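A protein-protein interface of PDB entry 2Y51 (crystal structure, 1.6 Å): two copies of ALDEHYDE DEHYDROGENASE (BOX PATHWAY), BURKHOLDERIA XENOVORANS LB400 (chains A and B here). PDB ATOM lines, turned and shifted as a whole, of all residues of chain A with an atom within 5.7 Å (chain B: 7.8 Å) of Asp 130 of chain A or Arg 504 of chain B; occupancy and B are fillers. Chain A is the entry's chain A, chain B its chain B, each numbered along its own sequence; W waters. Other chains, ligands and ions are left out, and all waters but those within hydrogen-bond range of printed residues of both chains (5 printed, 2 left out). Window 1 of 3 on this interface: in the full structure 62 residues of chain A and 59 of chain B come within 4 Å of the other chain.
Of chain B, only Arg 504 comes within 4 Å of Asp 130 of chain A. No residue of chain B comes within 4 Å of Gly 131 of chain A. Printed residues of chain B within 4 Å of Glu 134 of chain A: Met 485 (3.3 Å). Of the printed residues of chain B, Arg 512 of chain A touches Leu 487 and Glu 498. Of the printed residues of chain A, Met 485 of chain B touches Glu 134 (3.3 Å) and His 146 (3.5 Å). Of the printed residues of chain A, Ser 486 of chain B touches His 146. Printed residues of chain A within 4 Å of Glu 498 of chain B: Arg 512 (2.7 Å). Of chain A, only Asp 130 and His 146 come within 4 Å of Arg 504 of chain B.
N of Leu 487 of chain B sits at hydrogen-bond distance from NE2 of His 146 of chain A. The guanidinium group of Arg 504 of chain B is in hydrogen-bond range of a ring nitrogen (ND1) of His 146 of chain A (3.3 Å). OD2 of Asp 130 of chain A lies within salt-bridge range of NE of Arg 504 of chain B (3.0 Å). OE1 of Glu 498 of chain B is in salt-bridge range of NH1 of Arg 512 of chain A, 2.7 Å away.
Hydrophobic or aromatic side chains of chain B that line the printed part of chain A: Met 485 and Leu 487. Of the 12 printed residues of chain A, 4 touch a printed residue of chain B. Hydrophobic or aromatic side chains of chain A that line the printed part of chain B: His 146. Among the printed residues, Asp or Glu carboxylates within 4 Å of a Lys or Arg side-chain nitrogen of the other chain: Asp 130 of chain A with Arg 504 of chain B and Arg 512 of chain A with Glu 498 of chain B.
OE2 of Glu 134 of chain A touches CB of Met 485 of chain B (3.3 Å). CE1 of His 146 of chain A touches O of Met 485 of chain B, at 3.5 Å. His 146 of chain A touches Ser 486 of chain B. O of Arg 512 of chain A touches CD2 of Leu 487 of chain B (3.4 Å).
Water W3 bridges the side-chain hydroxyl (OH) of Tyr 114 of chain B (2.5 Å) and the side-chain carboxylate (OE2) of Glu 134 of chain A (2.9 Å). Water W4 lies within hydrogen-bond range of the side-chain carboxylate of Glu 498 of chain B (2.7 Å) and the backbone NH of Arg 512 of chain A (3.0 Å). Water W1 bridges O of Arg 512 of chain A (2.9 Å) and OE2 of Glu 498 of chain B (3.1 Å). Water W5 lies within hydrogen-bond range of O of Met 485 of chain B, OG of Ser 486 of chain B and OE1 of Glu 134 of chain A. Water W2 lies within hydrogen-bond range of OE1 of Glu 134 of chain A, NH2 of Arg 504 of chain B and O of Ser 132 of chain A.
The side-chain carboxylate of Asp 130 of chain A lies within salt-bridge range of the guanidinium group of Arg 512 of chain A (2.8 Å). The backbone carbonyl oxygen of Gly 501 of chain B lies within hydrogen-bond range of the guanidinium group of Arg 504 of chain B (3.0 Å). O of His 146 of chain A lies within hydrogen-bond range of N of Asp 130 of chain A (2.9 Å). The backbone carbonyl oxygen (O) of Ser 486 of chain B sits at hydrogen-bond distance from the backbone NH (N) of Gly 501 of chain B, at 3.0 Å.
Positions printed for both chains: 148, 512 and 531. Of the 8 pairs that touch across the chains among the printed residues, none has its exchanged pair printed and touching as well.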
ATOM      1  N   LEU A 128      11.328  -9.711 -28.894  1.00  0.00           N
ATOM      2  CA  LEU A 128      12.357  -8.662 -28.700  1.00  0.00           C
ATOM      3  C   LEU A 128      12.926  -8.764 -27.289  1.00  0.00           C
ATOM      4  O   LEU A 128      12.228  -9.220 -26.373  1.00  0.00           O
ATOM      5  CB  LEU A 128      11.723  -7.249 -28.872  1.00  0.00           C
ATOM      6  CG  LEU A 128      10.997  -6.900 -30.210  1.00  0.00           C
ATOM      7  CD1 LEU A 128      10.448  -5.475 -30.192  1.00  0.00           C
ATOM      8  CD2 LEU A 128      12.030  -7.096 -31.402  1.00  0.00           C
ATOM      9  N   ARG A 129      14.180  -8.381 -27.107  1.00  0.00           N
ATOM     10  CA  ARG A 129      14.753  -8.240 -25.740  1.00  0.00           C
ATOM     11  C   ARG A 129      14.492  -6.804 -25.188  1.00  0.00           C
ATOM     12  O   ARG A 129      14.548  -5.802 -25.919  1.00  0.00           O
ATOM     13  CB  ARG A 129      16.279  -8.521 -25.713  1.00  0.00           C
ATOM     14  CG  ARG A 129      16.483  -9.901 -26.162  1.00  0.00           C
ATOM     15  CD  ARG A 129      17.856 -10.475 -25.930  1.00  0.00           C
ATOM     16  NE  ARG A 129      18.421 -10.662 -27.253  1.00  0.00           N
ATOM     17  CZ  ARG A 129      19.507 -10.029 -27.682  1.00  0.00           C
ATOM     18  NH1 ARG A 129      20.168  -9.195 -26.870  1.00  0.00           N
ATOM     19  NH2 ARG A 129      19.949 -10.256 -28.908  1.00  0.00           N
ATOM     20  N   ASP A 130      14.124  -6.752 -23.922  1.00  0.00           N
ATOM     21  CA  ASP A 130      13.913  -5.504 -23.222  1.00  0.00           C
ATOM     22  C   ASP A 130      15.148  -5.364 -22.329  1.00  0.00           C
ATOM     23  O   ASP A 130      15.230  -5.962 -21.259  1.00  0.00           O
ATOM     24  CB  ASP A 130      12.624  -5.542 -22.433  1.00  0.00           C
ATOM     25  CG  ASP A 130      12.549  -4.424 -21.364  1.00  0.00           C
ATOM     26  OD1 ASP A 130      13.453  -3.598 -21.279  1.00  0.00           O
ATOM     27  OD2 ASP A 130      11.593  -4.351 -20.583  1.00  0.00           O
ATOM     28  N   GLY A 131      16.139  -4.605 -22.799  1.00  0.00           N
ATOM     29  CA  GLY A 131      17.274  -4.308 -21.927  1.00  0.00           C
ATOM     30  C   GLY A 131      18.250  -5.498 -21.976  1.00  0.00           C
ATOM     31  O   GLY A 131      18.128  -6.463 -22.778  1.00  0.00           O
ATOM     32  N   SER A 132      19.259  -5.425 -21.128  1.00  0.00           N
ATOM     33  CA  SER A 132      20.186  -6.523 -21.149  1.00  0.00           C
ATOM     34  C   SER A 132      19.990  -7.504 -20.013  1.00  0.00           C
ATOM     35  O   SER A 132      19.191  -7.289 -19.059  1.00  0.00           O
ATOM     36  CB  SER A 132      21.603  -6.023 -21.146  1.00  0.00           C
ATOM     37  OG  SER A 132      21.724  -5.125 -20.076  1.00  0.00           O
ATOM     38  N   GLU A 134      21.074  -9.780 -16.863  1.00  0.00           N
ATOM     39  CA  GLU A 134      21.400  -9.301 -15.565  1.00  0.00           C
ATOM     40  C   GLU A 134      21.595 -10.509 -14.624  1.00  0.00           C
ATOM     41  O   GLU A 134      20.873 -11.472 -14.714  1.00  0.00           O
ATOM     42  CB  GLU A 134      20.242  -8.402 -15.125  1.00  0.00           C
ATOM     43  CG  GLU A 134      20.125  -8.207 -13.710  1.00  0.00           C
ATOM     44  CD  GLU A 134      19.482  -6.862 -13.322  1.00  0.00           C
ATOM     45  OE1 GLU A 134      18.592  -6.351 -14.044  1.00  0.00           O
ATOM     46  OE2 GLU A 134      19.818  -6.392 -12.231  1.00  0.00           O
ATOM     47  N   GLN A 145      16.620 -12.206 -18.193  1.00  0.00           N
ATOM     48  CA  GLN A 145      16.490 -11.354 -19.367  1.00  0.00           C
ATOM     49  C   GLN A 145      15.008 -11.129 -19.562  1.00  0.00           C
ATOM     50  O   GLN A 145      14.260 -12.089 -19.638  1.00  0.00           O
ATOM     51  CB  GLN A 145      17.058 -12.097 -20.631  1.00  0.00           C
ATOM     52  CG  GLN A 145      16.790 -11.396 -22.006  1.00  0.00           C
ATOM     53  CD  GLN A 145      17.532 -10.066 -22.169  1.00  0.00           C
ATOM     54  OE1 GLN A 145      18.774 -10.026 -22.150  1.00  0.00           O
ATOM     55  NE2 GLN A 145      16.791  -8.959 -22.269  1.00  0.00           N
ATOM     56  N   HIS A 146      14.603  -9.851 -19.654  1.00  0.00           N
ATOM     57  CA  HIS A 146      13.247  -9.493 -19.974  1.00  0.00           C
ATOM     58  C   HIS A 146      13.041  -9.554 -21.502  1.00  0.00           C
ATOM     59  O   HIS A 146      13.952  -9.176 -22.298  1.00  0.00           O
ATOM     60  CB  HIS A 146      12.985  -8.029 -19.510  1.00  0.00           C
ATOM     61  CG  HIS A 146      13.013  -7.886 -18.020  1.00  0.00           C
ATOM     62  ND1 HIS A 146      14.180  -7.845 -17.270  1.00  0.00           N
ATOM     63  CD2 HIS A 146      11.989  -7.884 -17.126  1.00  0.00           C
ATOM     64  CE1 HIS A 146      13.865  -7.766 -15.981  1.00  0.00           C
ATOM     65  NE2 HIS A 146      12.538  -7.759 -15.873  1.00  0.00           N
ATOM     66  N   VAL A 147      11.839  -9.935 -21.894  1.00  0.00           N
ATOM     67  CA  VAL A 147      11.487 -10.015 -23.335  1.00  0.00           C
ATOM     68  C   VAL A 147      10.131  -9.386 -23.588  1.00  0.00           C
ATOM     69  O   VAL A 147       9.406  -9.123 -22.617  1.00  0.00           O
ATOM     70  CB  VAL A 147      11.508 -11.509 -23.847  1.00  0.00           C
ATOM     71  CG1 VAL A 147      12.986 -12.137 -23.708  1.00  0.00           C
ATOM     72  CG2 VAL A 147      10.450 -12.378 -23.172  1.00  0.00           C
ATOM     73  N   LEU A 148       9.816  -9.095 -24.853  1.00  0.00           N
ATOM     74  CA  LEU A 148       8.493  -8.578 -25.251  1.00  0.00           C
ATOM     75  C   LEU A 148       7.970  -9.497 -26.297  1.00  0.00           C
ATOM     76  O   LEU A 148       8.671  -9.739 -27.280  1.00  0.00           O
ATOM     77  CB  LEU A 148       8.629  -7.158 -25.863  1.00  0.00           C
ATOM     78  CG  LEU A 148       9.019  -6.104 -24.847  1.00  0.00           C
ATOM     79  CD1 LEU A 148       9.633  -4.789 -25.496  1.00  0.00           C
ATOM     80  CD2 LEU A 148       7.825  -5.761 -24.073  1.00  0.00           C
ATOM     81  N   ARG A 512       5.304  -8.061 -21.654  1.00  0.00           N
ATOM     82  CA  ARG A 512       6.694  -8.047 -21.145  1.00  0.00           C
ATOM     83  C   ARG A 512       6.827  -9.179 -20.103  1.00  0.00           C
ATOM     84  O   ARG A 512       5.930  -9.402 -19.279  1.00  0.00           O
ATOM     85  CB  ARG A 512       6.987  -6.706 -20.466  1.00  0.00           C
ATOM     86  CG  ARG A 512       8.456  -6.512 -20.015  1.00  0.00           C
ATOM     87  CD  ARG A 512       8.635  -5.176 -19.277  1.00  0.00           C
ATOM     88  NE  ARG A 512       8.844  -4.101 -20.233  1.00  0.00           N
ATOM     89  CZ  ARG A 512       7.880  -3.312 -20.687  1.00  0.00           C
ATOM     90  NH1 ARG A 512       6.673  -3.452 -20.198  1.00  0.00           N
ATOM     91  NH2 ARG A 512       8.099  -2.412 -21.655  1.00  0.00           N
ATOM     92  N   TRP A 531      17.568  -7.287 -29.632  1.00  0.00           N
ATOM     93  CA  TRP A 531      17.627  -6.228 -28.671  1.00  0.00           C
ATOM     94  C   TRP A 531      17.760  -4.899 -29.445  1.00  0.00           C
ATOM     95  O   TRP A 531      18.883  -4.466 -29.752  1.00  0.00           O
ATOM     96  CB  TRP A 531      18.839  -6.519 -27.720  1.00  0.00           C
ATOM     97  CG  TRP A 531      19.157  -5.527 -26.648  1.00  0.00           C
ATOM     98  CD1 TRP A 531      20.322  -5.451 -25.942  1.00  0.00           C
ATOM     99  CD2 TRP A 531      18.319  -4.452 -26.179  1.00  0.00           C
ATOM    100  NE1 TRP A 531      20.257  -4.402 -25.041  1.00  0.00           N
ATOM    101  CE2 TRP A 531      19.054  -3.758 -25.178  1.00  0.00           C
ATOM    102  CE3 TRP A 531      17.035  -3.982 -26.528  1.00  0.00           C
ATOM    103  CZ2 TRP A 531      18.535  -2.623 -24.489  1.00  0.00           C
ATOM    104  CZ3 TRP A 531      16.516  -2.836 -25.850  1.00  0.00           C
ATOM    105  CH2 TRP A 531      17.283  -2.173 -24.843  1.00  0.00           C
ATOM    106  N   TYR B 114      18.158  -2.606  -2.388  1.00  0.00           N
ATOM    107  CA  TYR B 114      18.368  -2.653  -3.836  1.00  0.00           C
ATOM    108  C   TYR B 114      18.019  -1.301  -4.478  1.00  0.00           C
ATOM    109  O   TYR B 114      18.795  -0.696  -5.195  1.00  0.00           O
ATOM    110  CB  TYR B 114      17.574  -3.795  -4.437  1.00  0.00           C
ATOM    111  CG  TYR B 114      17.522  -3.762  -5.935  1.00  0.00           C
ATOM    112  CD1 TYR B 114      18.683  -4.047  -6.733  1.00  0.00           C
ATOM    113  CD2 TYR B 114      16.373  -3.387  -6.596  1.00  0.00           C
ATOM    114  CE1 TYR B 114      18.602  -4.027  -8.194  1.00  0.00           C
ATOM    115  CE2 TYR B 114      16.317  -3.330  -8.010  1.00  0.00           C
ATOM    116  CZ  TYR B 114      17.392  -3.684  -8.793  1.00  0.00           C
ATOM    117  OH  TYR B 114      17.242  -3.604 -10.131  1.00  0.00           O
ATOM    118  N   TYR B 115      16.825  -0.760  -4.190  1.00  0.00           N
ATOM    119  CA  TYR B 115      16.489   0.512  -4.764  1.00  0.00           C
ATOM    120  C   TYR B 115      17.292   1.722  -4.210  1.00  0.00           C
ATOM    121  O   TYR B 115      17.524   2.702  -4.949  1.00  0.00           O
ATOM    122  CB  TYR B 115      14.948   0.779  -4.570  1.00  0.00           C
ATOM    123  CG  TYR B 115      14.159   0.122  -5.697  1.00  0.00           C
ATOM    124  CD1 TYR B 115      14.027   0.779  -6.959  1.00  0.00           C
ATOM    125  CD2 TYR B 115      13.658  -1.198  -5.573  1.00  0.00           C
ATOM    126  CE1 TYR B 115      13.407   0.134  -8.050  1.00  0.00           C
ATOM    127  CE2 TYR B 115      13.015  -1.871  -6.620  1.00  0.00           C
ATOM    128  CZ  TYR B 115      12.839  -1.197  -7.864  1.00  0.00           C
ATOM    129  OH  TYR B 115      12.284  -1.862  -8.922  1.00  0.00           O
ATOM    130  N   LEU B 118      20.420   1.443  -6.276  1.00  0.00           N
ATOM    131  CA  LEU B 118      20.137   1.810  -7.675  1.00  0.00           C
ATOM    132  C   LEU B 118      19.892   3.300  -7.752  1.00  0.00           C
ATOM    133  O   LEU B 118      20.255   3.991  -8.726  1.00  0.00           O
ATOM    134  CB  LEU B 118      18.869   1.050  -8.092  1.00  0.00           C
ATOM    135  CG  LEU B 118      18.476   0.870  -9.535  1.00  0.00           C
ATOM    136  CD1 LEU B 118      19.532   0.081 -10.264  1.00  0.00           C
ATOM    137  CD2 LEU B 118      17.075   0.111  -9.551  1.00  0.00           C
ATOM    138  N   LEU B 148      11.571  11.918 -18.324  1.00  0.00           N
ATOM    139  CA  LEU B 148      10.648  11.396 -17.287  1.00  0.00           C
ATOM    140  C   LEU B 148      10.645  12.341 -16.119  1.00  0.00           C
ATOM    141  O   LEU B 148      11.692  12.636 -15.548  1.00  0.00           O
ATOM    142  CB  LEU B 148      11.097  10.016 -16.791  1.00  0.00           C
ATOM    143  CG  LEU B 148      11.019   8.909 -17.834  1.00  0.00           C
ATOM    144  CD1 LEU B 148      11.794   7.600 -17.375  1.00  0.00           C
ATOM    145  CD2 LEU B 148       9.596   8.544 -18.174  1.00  0.00           C
ATOM    146  N   PRO B 174      10.536   2.440  -5.081  1.00  0.00           N
ATOM    147  CA  PRO B 174      10.572   3.209  -6.347  1.00  0.00           C
ATOM    148  C   PRO B 174       9.690   4.469  -6.339  1.00  0.00           C
ATOM    149  O   PRO B 174       9.985   5.428  -6.994  1.00  0.00           O
ATOM    150  CB  PRO B 174       9.997   2.177  -7.432  1.00  0.00           C
ATOM    151  CG  PRO B 174       9.277   1.112  -6.622  1.00  0.00           C
ATOM    152  CD  PRO B 174      10.016   1.066  -5.272  1.00  0.00           C
ATOM    153  N   PRO B 484      13.784  -8.156  -6.957  1.00  0.00           N
ATOM    154  CA  PRO B 484      13.353  -6.775  -7.288  1.00  0.00           C
ATOM    155  C   PRO B 484      13.872  -6.265  -8.677  1.00  0.00           C
ATOM    156  O   PRO B 484      13.291  -5.342  -9.285  1.00  0.00           O
ATOM    157  CB  PRO B 484      13.826  -5.986  -6.100  1.00  0.00           C
ATOM    158  CG  PRO B 484      15.155  -6.711  -5.725  1.00  0.00           C
ATOM    159  CD  PRO B 484      14.740  -8.184  -5.829  1.00  0.00           C
ATOM    160  N   MET B 485      14.968  -6.868  -9.164  1.00  0.00           N
ATOM    161  CA  MET B 485      15.489  -6.481 -10.484  1.00  0.00           C
ATOM    162  C   MET B 485      14.651  -7.102 -11.628  1.00  0.00           C
ATOM    163  O   MET B 485      14.835  -6.738 -12.821  1.00  0.00           O
ATOM    164  CB  MET B 485      16.966  -6.933 -10.620  1.00  0.00           C
ATOM    165  CG  MET B 485      17.137  -8.345 -10.390  1.00  0.00           C
ATOM    166  SD  MET B 485      17.451  -8.768  -8.658  1.00  0.00           S
ATOM    167  CE  MET B 485      18.834  -7.777  -8.200  1.00  0.00           C
ATOM    168  N   SER B 486      13.701  -7.987 -11.260  1.00  0.00           N
ATOM    169  CA  SER B 486      12.882  -8.648 -12.277  1.00  0.00           C
ATOM    170  C   SER B 486      11.421  -8.213 -12.233  1.00  0.00           C
ATOM    171  O   SER B 486      10.871  -7.986 -11.178  1.00  0.00           O
ATOM    172  CB  SER B 486      12.990 -10.171 -12.109  1.00  0.00           C
ATOM    173  OG  SER B 486      14.308 -10.654 -12.471  1.00  0.00           O
ATOM    174  N   LEU B 487      10.762  -8.149 -13.378  1.00  0.00           N
ATOM    175  CA  LEU B 487       9.362  -7.778 -13.418  1.00  0.00           C
ATOM    176  C   LEU B 487       8.513  -8.642 -12.515  1.00  0.00           C
ATOM    177  O   LEU B 487       8.714  -9.879 -12.452  1.00  0.00           O
ATOM    178  CB  LEU B 487       8.898  -7.905 -14.860  1.00  0.00           C
ATOM    179  CG  LEU B 487       7.411  -7.571 -15.103  1.00  0.00           C
ATOM    180  CD1 LEU B 487       7.215  -6.127 -14.995  1.00  0.00           C
ATOM    181  CD2 LEU B 487       7.274  -7.929 -16.542  1.00  0.00           C
ATOM    182  N   GLU B 498       2.293  -4.250 -13.830  1.00  0.00           N
ATOM    183  CA  GLU B 498       3.795  -4.362 -13.848  1.00  0.00           C
ATOM    184  C   GLU B 498       4.357  -3.542 -12.664  1.00  0.00           C
ATOM    185  O   GLU B 498       4.045  -2.316 -12.529  1.00  0.00           O
ATOM    186  CB  GLU B 498       4.326  -3.816 -15.205  1.00  0.00           C
ATOM    187  CG  GLU B 498       4.009  -4.723 -16.355  1.00  0.00           C
ATOM    188  CD  GLU B 498       4.666  -4.374 -17.682  1.00  0.00           C
ATOM    189  OE1 GLU B 498       5.786  -3.881 -17.683  1.00  0.00           O
ATOM    190  OE2 GLU B 498       4.151  -4.744 -18.749  1.00  0.00           O
ATOM    191  N   GLU B 499       5.236  -4.144 -11.863  1.00  0.00           N
ATOM    192  CA  GLU B 499       5.945  -3.355 -10.865  1.00  0.00           C
ATOM    193  C   GLU B 499       7.324  -3.961 -10.777  1.00  0.00           C
ATOM    194  O   GLU B 499       7.611  -4.939 -11.509  1.00  0.00           O
ATOM    195  CB  GLU B 499       5.257  -3.314  -9.479  1.00  0.00           C
ATOM    196  CG  GLU B 499       5.186  -4.606  -8.733  1.00  0.00           C
ATOM    197  CD  GLU B 499       4.899  -4.406  -7.234  1.00  0.00           C
ATOM    198  OE1 GLU B 499       5.757  -3.916  -6.481  1.00  0.00           O
ATOM    199  OE2 GLU B 499       3.814  -4.767  -6.808  1.00  0.00           O
ATOM    200  N   LEU B 500       8.163  -3.422  -9.902  1.00  0.00           N
ATOM    201  CA  LEU B 500       9.580  -3.874  -9.782  1.00  0.00           C
ATOM    202  C   LEU B 500      10.273  -3.934 -11.178  1.00  0.00           C
ATOM    203  O   LEU B 500      10.076  -2.999 -11.982  1.00  0.00           O
ATOM    204  CB  LEU B 500       9.713  -5.191  -9.043  1.00  0.00           C
ATOM    205  CG  LEU B 500       9.188  -5.089  -7.610  1.00  0.00           C
ATOM    206  CD1 LEU B 500       9.026  -6.432  -6.924  1.00  0.00           C
ATOM    207  CD2 LEU B 500      10.041  -4.184  -6.757  1.00  0.00           C
ATOM    208  N   GLY B 501      11.079  -4.958 -11.440  1.00  0.00           N
ATOM    209  CA  GLY B 501      11.870  -5.001 -12.707  1.00  0.00           C
ATOM    210  C   GLY B 501      12.937  -3.870 -12.663  1.00  0.00           C
ATOM    211  O   GLY B 501      13.309  -3.249 -13.706  1.00  0.00           O
ATOM    212  N   GLY B 502      13.477  -3.625 -11.484  1.00  0.00           N
ATOM    213  CA  GLY B 502      14.543  -2.652 -11.327  1.00  0.00           C
ATOM    214  C   GLY B 502      14.133  -1.235 -11.711  1.00  0.00           C
ATOM    215  O   GLY B 502      13.166  -0.719 -11.188  1.00  0.00           O
ATOM    216  N   LEU B 503      14.891  -0.572 -12.582  1.00  0.00           N
ATOM    217  CA  LEU B 503      14.573   0.813 -13.049  1.00  0.00           C
ATOM    218  C   LEU B 503      13.182   0.882 -13.694  1.00  0.00           C
ATOM    219  O   LEU B 503      12.671   1.982 -13.803  1.00  0.00           O
ATOM    220  CB  LEU B 503      15.584   1.330 -14.093  1.00  0.00           C
ATOM    221  CG  LEU B 503      17.006   1.399 -13.543  1.00  0.00           C
ATOM    222  CD1 LEU B 503      18.155   1.502 -14.539  1.00  0.00           C
ATOM    223  CD2 LEU B 503      17.153   2.490 -12.459  1.00  0.00           C
ATOM    224  N   ARG B 504      12.680  -0.248 -14.212  1.00  0.00           N
ATOM    225  CA  ARG B 504      11.380  -0.275 -14.951  1.00  0.00           C
ATOM    226  C   ARG B 504      10.273   0.228 -14.061  1.00  0.00           C
ATOM    227  O   ARG B 504       9.263   0.879 -14.511  1.00  0.00           O
ATOM    228  CB  ARG B 504      11.039  -1.692 -15.513  1.00  0.00           C
ATOM    229  CG  ARG B 504      12.029  -2.145 -16.594  1.00  0.00           C
ATOM    230  CD  ARG B 504      11.818  -3.556 -16.945  1.00  0.00           C
ATOM    231  NE  ARG B 504      12.824  -4.058 -17.901  1.00  0.00           N
ATOM    232  CZ  ARG B 504      14.037  -4.430 -17.525  1.00  0.00           C
ATOM    233  NH1 ARG B 504      14.442  -4.360 -16.242  1.00  0.00           N
ATOM    234  NH2 ARG B 504      14.857  -4.861 -18.449  1.00  0.00           N
ATOM    235  N   ALA B 505      10.480   0.046 -12.764  1.00  0.00           N
ATOM    236  CA  ALA B 505       9.418   0.409 -11.784  1.00  0.00           C
ATOM    237  C   ALA B 505       9.230   1.921 -11.691  1.00  0.00           C
ATOM    238  O   ALA B 505       8.163   2.410 -11.283  1.00  0.00           O
ATOM    239  CB  ALA B 505       9.680  -0.132 -10.373  1.00  0.00           C
ATOM    240  N   LEU B 506      10.223   2.678 -12.096  1.00  0.00           N
ATOM    241  CA  LEU B 506      10.138   4.134 -11.984  1.00  0.00           C
ATOM    242  C   LEU B 506       9.169   4.737 -12.911  1.00  0.00           C
ATOM    243  O   LEU B 506       8.626   5.778 -12.550  1.00  0.00           O
ATOM    244  CB  LEU B 506      11.512   4.806 -12.225  1.00  0.00           C
ATOM    245  CG  LEU B 506      12.644   4.396 -11.299  1.00  0.00           C
ATOM    246  CD1 LEU B 506      13.972   5.115 -11.740  1.00  0.00           C
ATOM    247  CD2 LEU B 506      12.399   4.535  -9.869  1.00  0.00           C
ATOM    248  N   ALA B 507       8.883   4.109 -14.050  1.00  0.00           N
ATOM    249  CA  ALA B 507       8.008   4.724 -15.076  1.00  0.00           C
ATOM    250  C   ALA B 507       6.616   4.988 -14.544  1.00  0.00           C
ATOM    251  O   ALA B 507       6.074   6.024 -14.907  1.00  0.00           O
ATOM    252  CB  ALA B 507       7.937   3.810 -16.407  1.00  0.00           C
ATOM    253  N   PHE B 508       6.101   4.085 -13.687  1.00  0.00           N
ATOM    254  CA  PHE B 508       4.742   4.157 -13.150  1.00  0.00           C
ATOM    255  C   PHE B 508       4.583   5.438 -12.365  1.00  0.00           C
ATOM    256  O   PHE B 508       3.433   5.969 -12.266  1.00  0.00           O
ATOM    257  CB  PHE B 508       4.499   2.951 -12.234  1.00  0.00           C
ATOM    258  CG  PHE B 508       3.113   2.845 -11.698  1.00  0.00           C
ATOM    259  CD1 PHE B 508       2.095   2.537 -12.563  1.00  0.00           C
ATOM    260  CD2 PHE B 508       2.881   2.983 -10.348  1.00  0.00           C
ATOM    261  CE1 PHE B 508       0.801   2.368 -12.064  1.00  0.00           C
ATOM    262  CE2 PHE B 508       1.548   2.821  -9.826  1.00  0.00           C
ATOM    263  CZ  PHE B 508       0.545   2.513 -10.706  1.00  0.00           C
ATOM    264  N   TYR B 509       5.679   5.980 -11.844  1.00  0.00           N
ATOM    265  CA  TYR B 509       5.609   7.194 -10.972  1.00  0.00           C
ATOM    266  C   TYR B 509       5.955   8.483 -11.735  1.00  0.00           C
ATOM    267  O   TYR B 509       5.984   9.574 -11.160  1.00  0.00           O
ATOM    268  CB  TYR B 509       6.467   7.013  -9.699  1.00  0.00           C
ATOM    269  CG  TYR B 509       6.031   5.820  -8.930  1.00  0.00           C
ATOM    270  CD1 TYR B 509       4.883   5.912  -8.072  1.00  0.00           C
ATOM    271  CD2 TYR B 509       6.680   4.594  -9.012  1.00  0.00           C
ATOM    272  CE1 TYR B 509       4.488   4.805  -7.367  1.00  0.00           C
ATOM    273  CE2 TYR B 509       6.244   3.460  -8.281  1.00  0.00           C
ATOM    274  CZ  TYR B 509       5.107   3.599  -7.497  1.00  0.00           C
ATOM    275  OH  TYR B 509       4.622   2.546  -6.813  1.00  0.00           O
ATOM    276  N   ARG B 512       6.042  10.802 -18.934  1.00  0.00           N
ATOM    277  CA  ARG B 512       7.010  10.863 -20.073  1.00  0.00           C
ATOM    278  C   ARG B 512       6.627  12.035 -20.971  1.00  0.00           C
ATOM    279  O   ARG B 512       5.401  12.281 -21.218  1.00  0.00           O
ATOM    280  CB  ARG B 512       6.970   9.538 -20.871  1.00  0.00           C
ATOM    281  CG  ARG B 512       8.094   9.408 -21.910  1.00  0.00           C
ATOM    282  CD  ARG B 512       8.025   7.942 -22.578  1.00  0.00           C
ATOM    283  NE  ARG B 512       7.541   6.852 -21.653  1.00  0.00           N
ATOM    284  CZ  ARG B 512       8.353   6.057 -20.982  1.00  0.00           C
ATOM    285  NH1 ARG B 512       9.651   6.191 -21.122  1.00  0.00           N
ATOM    286  NH2 ARG B 512       7.902   5.137 -20.186  1.00  0.00           N
ATOM    287  N   TRP B 531      20.567   9.381 -17.106  1.00  0.00           N
ATOM    288  CA  TRP B 531      20.168   7.934 -17.031  1.00  0.00           C
ATOM    289  C   TRP B 531      21.327   6.984 -16.895  1.00  0.00           C
ATOM    290  O   TRP B 531      22.362   7.201 -17.537  1.00  0.00           O
ATOM    291  CB  TRP B 531      19.401   7.515 -18.232  1.00  0.00           C
ATOM    292  CG  TRP B 531      18.791   6.133 -18.090  1.00  0.00           C
ATOM    293  CD1 TRP B 531      19.318   4.909 -18.569  1.00  0.00           C
ATOM    294  CD2 TRP B 531      17.541   5.802 -17.443  1.00  0.00           C
ATOM    295  NE1 TRP B 531      18.440   3.874 -18.262  1.00  0.00           N
ATOM    296  CE2 TRP B 531      17.349   4.379 -17.583  1.00  0.00           C
ATOM    297  CE3 TRP B 531      16.562   6.557 -16.761  1.00  0.00           C
ATOM    298  CZ2 TRP B 531      16.212   3.707 -17.054  1.00  0.00           C
ATOM    299  CZ3 TRP B 531      15.370   5.870 -16.258  1.00  0.00           C
ATOM    300  CH2 TRP B 531      15.234   4.473 -16.396  1.00  0.00           C
HETATM  301  O   HOH W   1       3.764  -7.765 -18.331  1.00  0.00           O
HETATM  302  O   HOH W   2      17.369  -5.623 -16.732  1.00  0.00           O
HETATM  303  O   HOH W   3      19.447  -3.611 -11.380  1.00  0.00           O
HETATM  304  O   HOH W   4       3.597  -5.674 -21.173  1.00  0.00           O
HETATM  305  O   HOH W   5      16.315  -9.003 -13.988  1.00  0.00           O
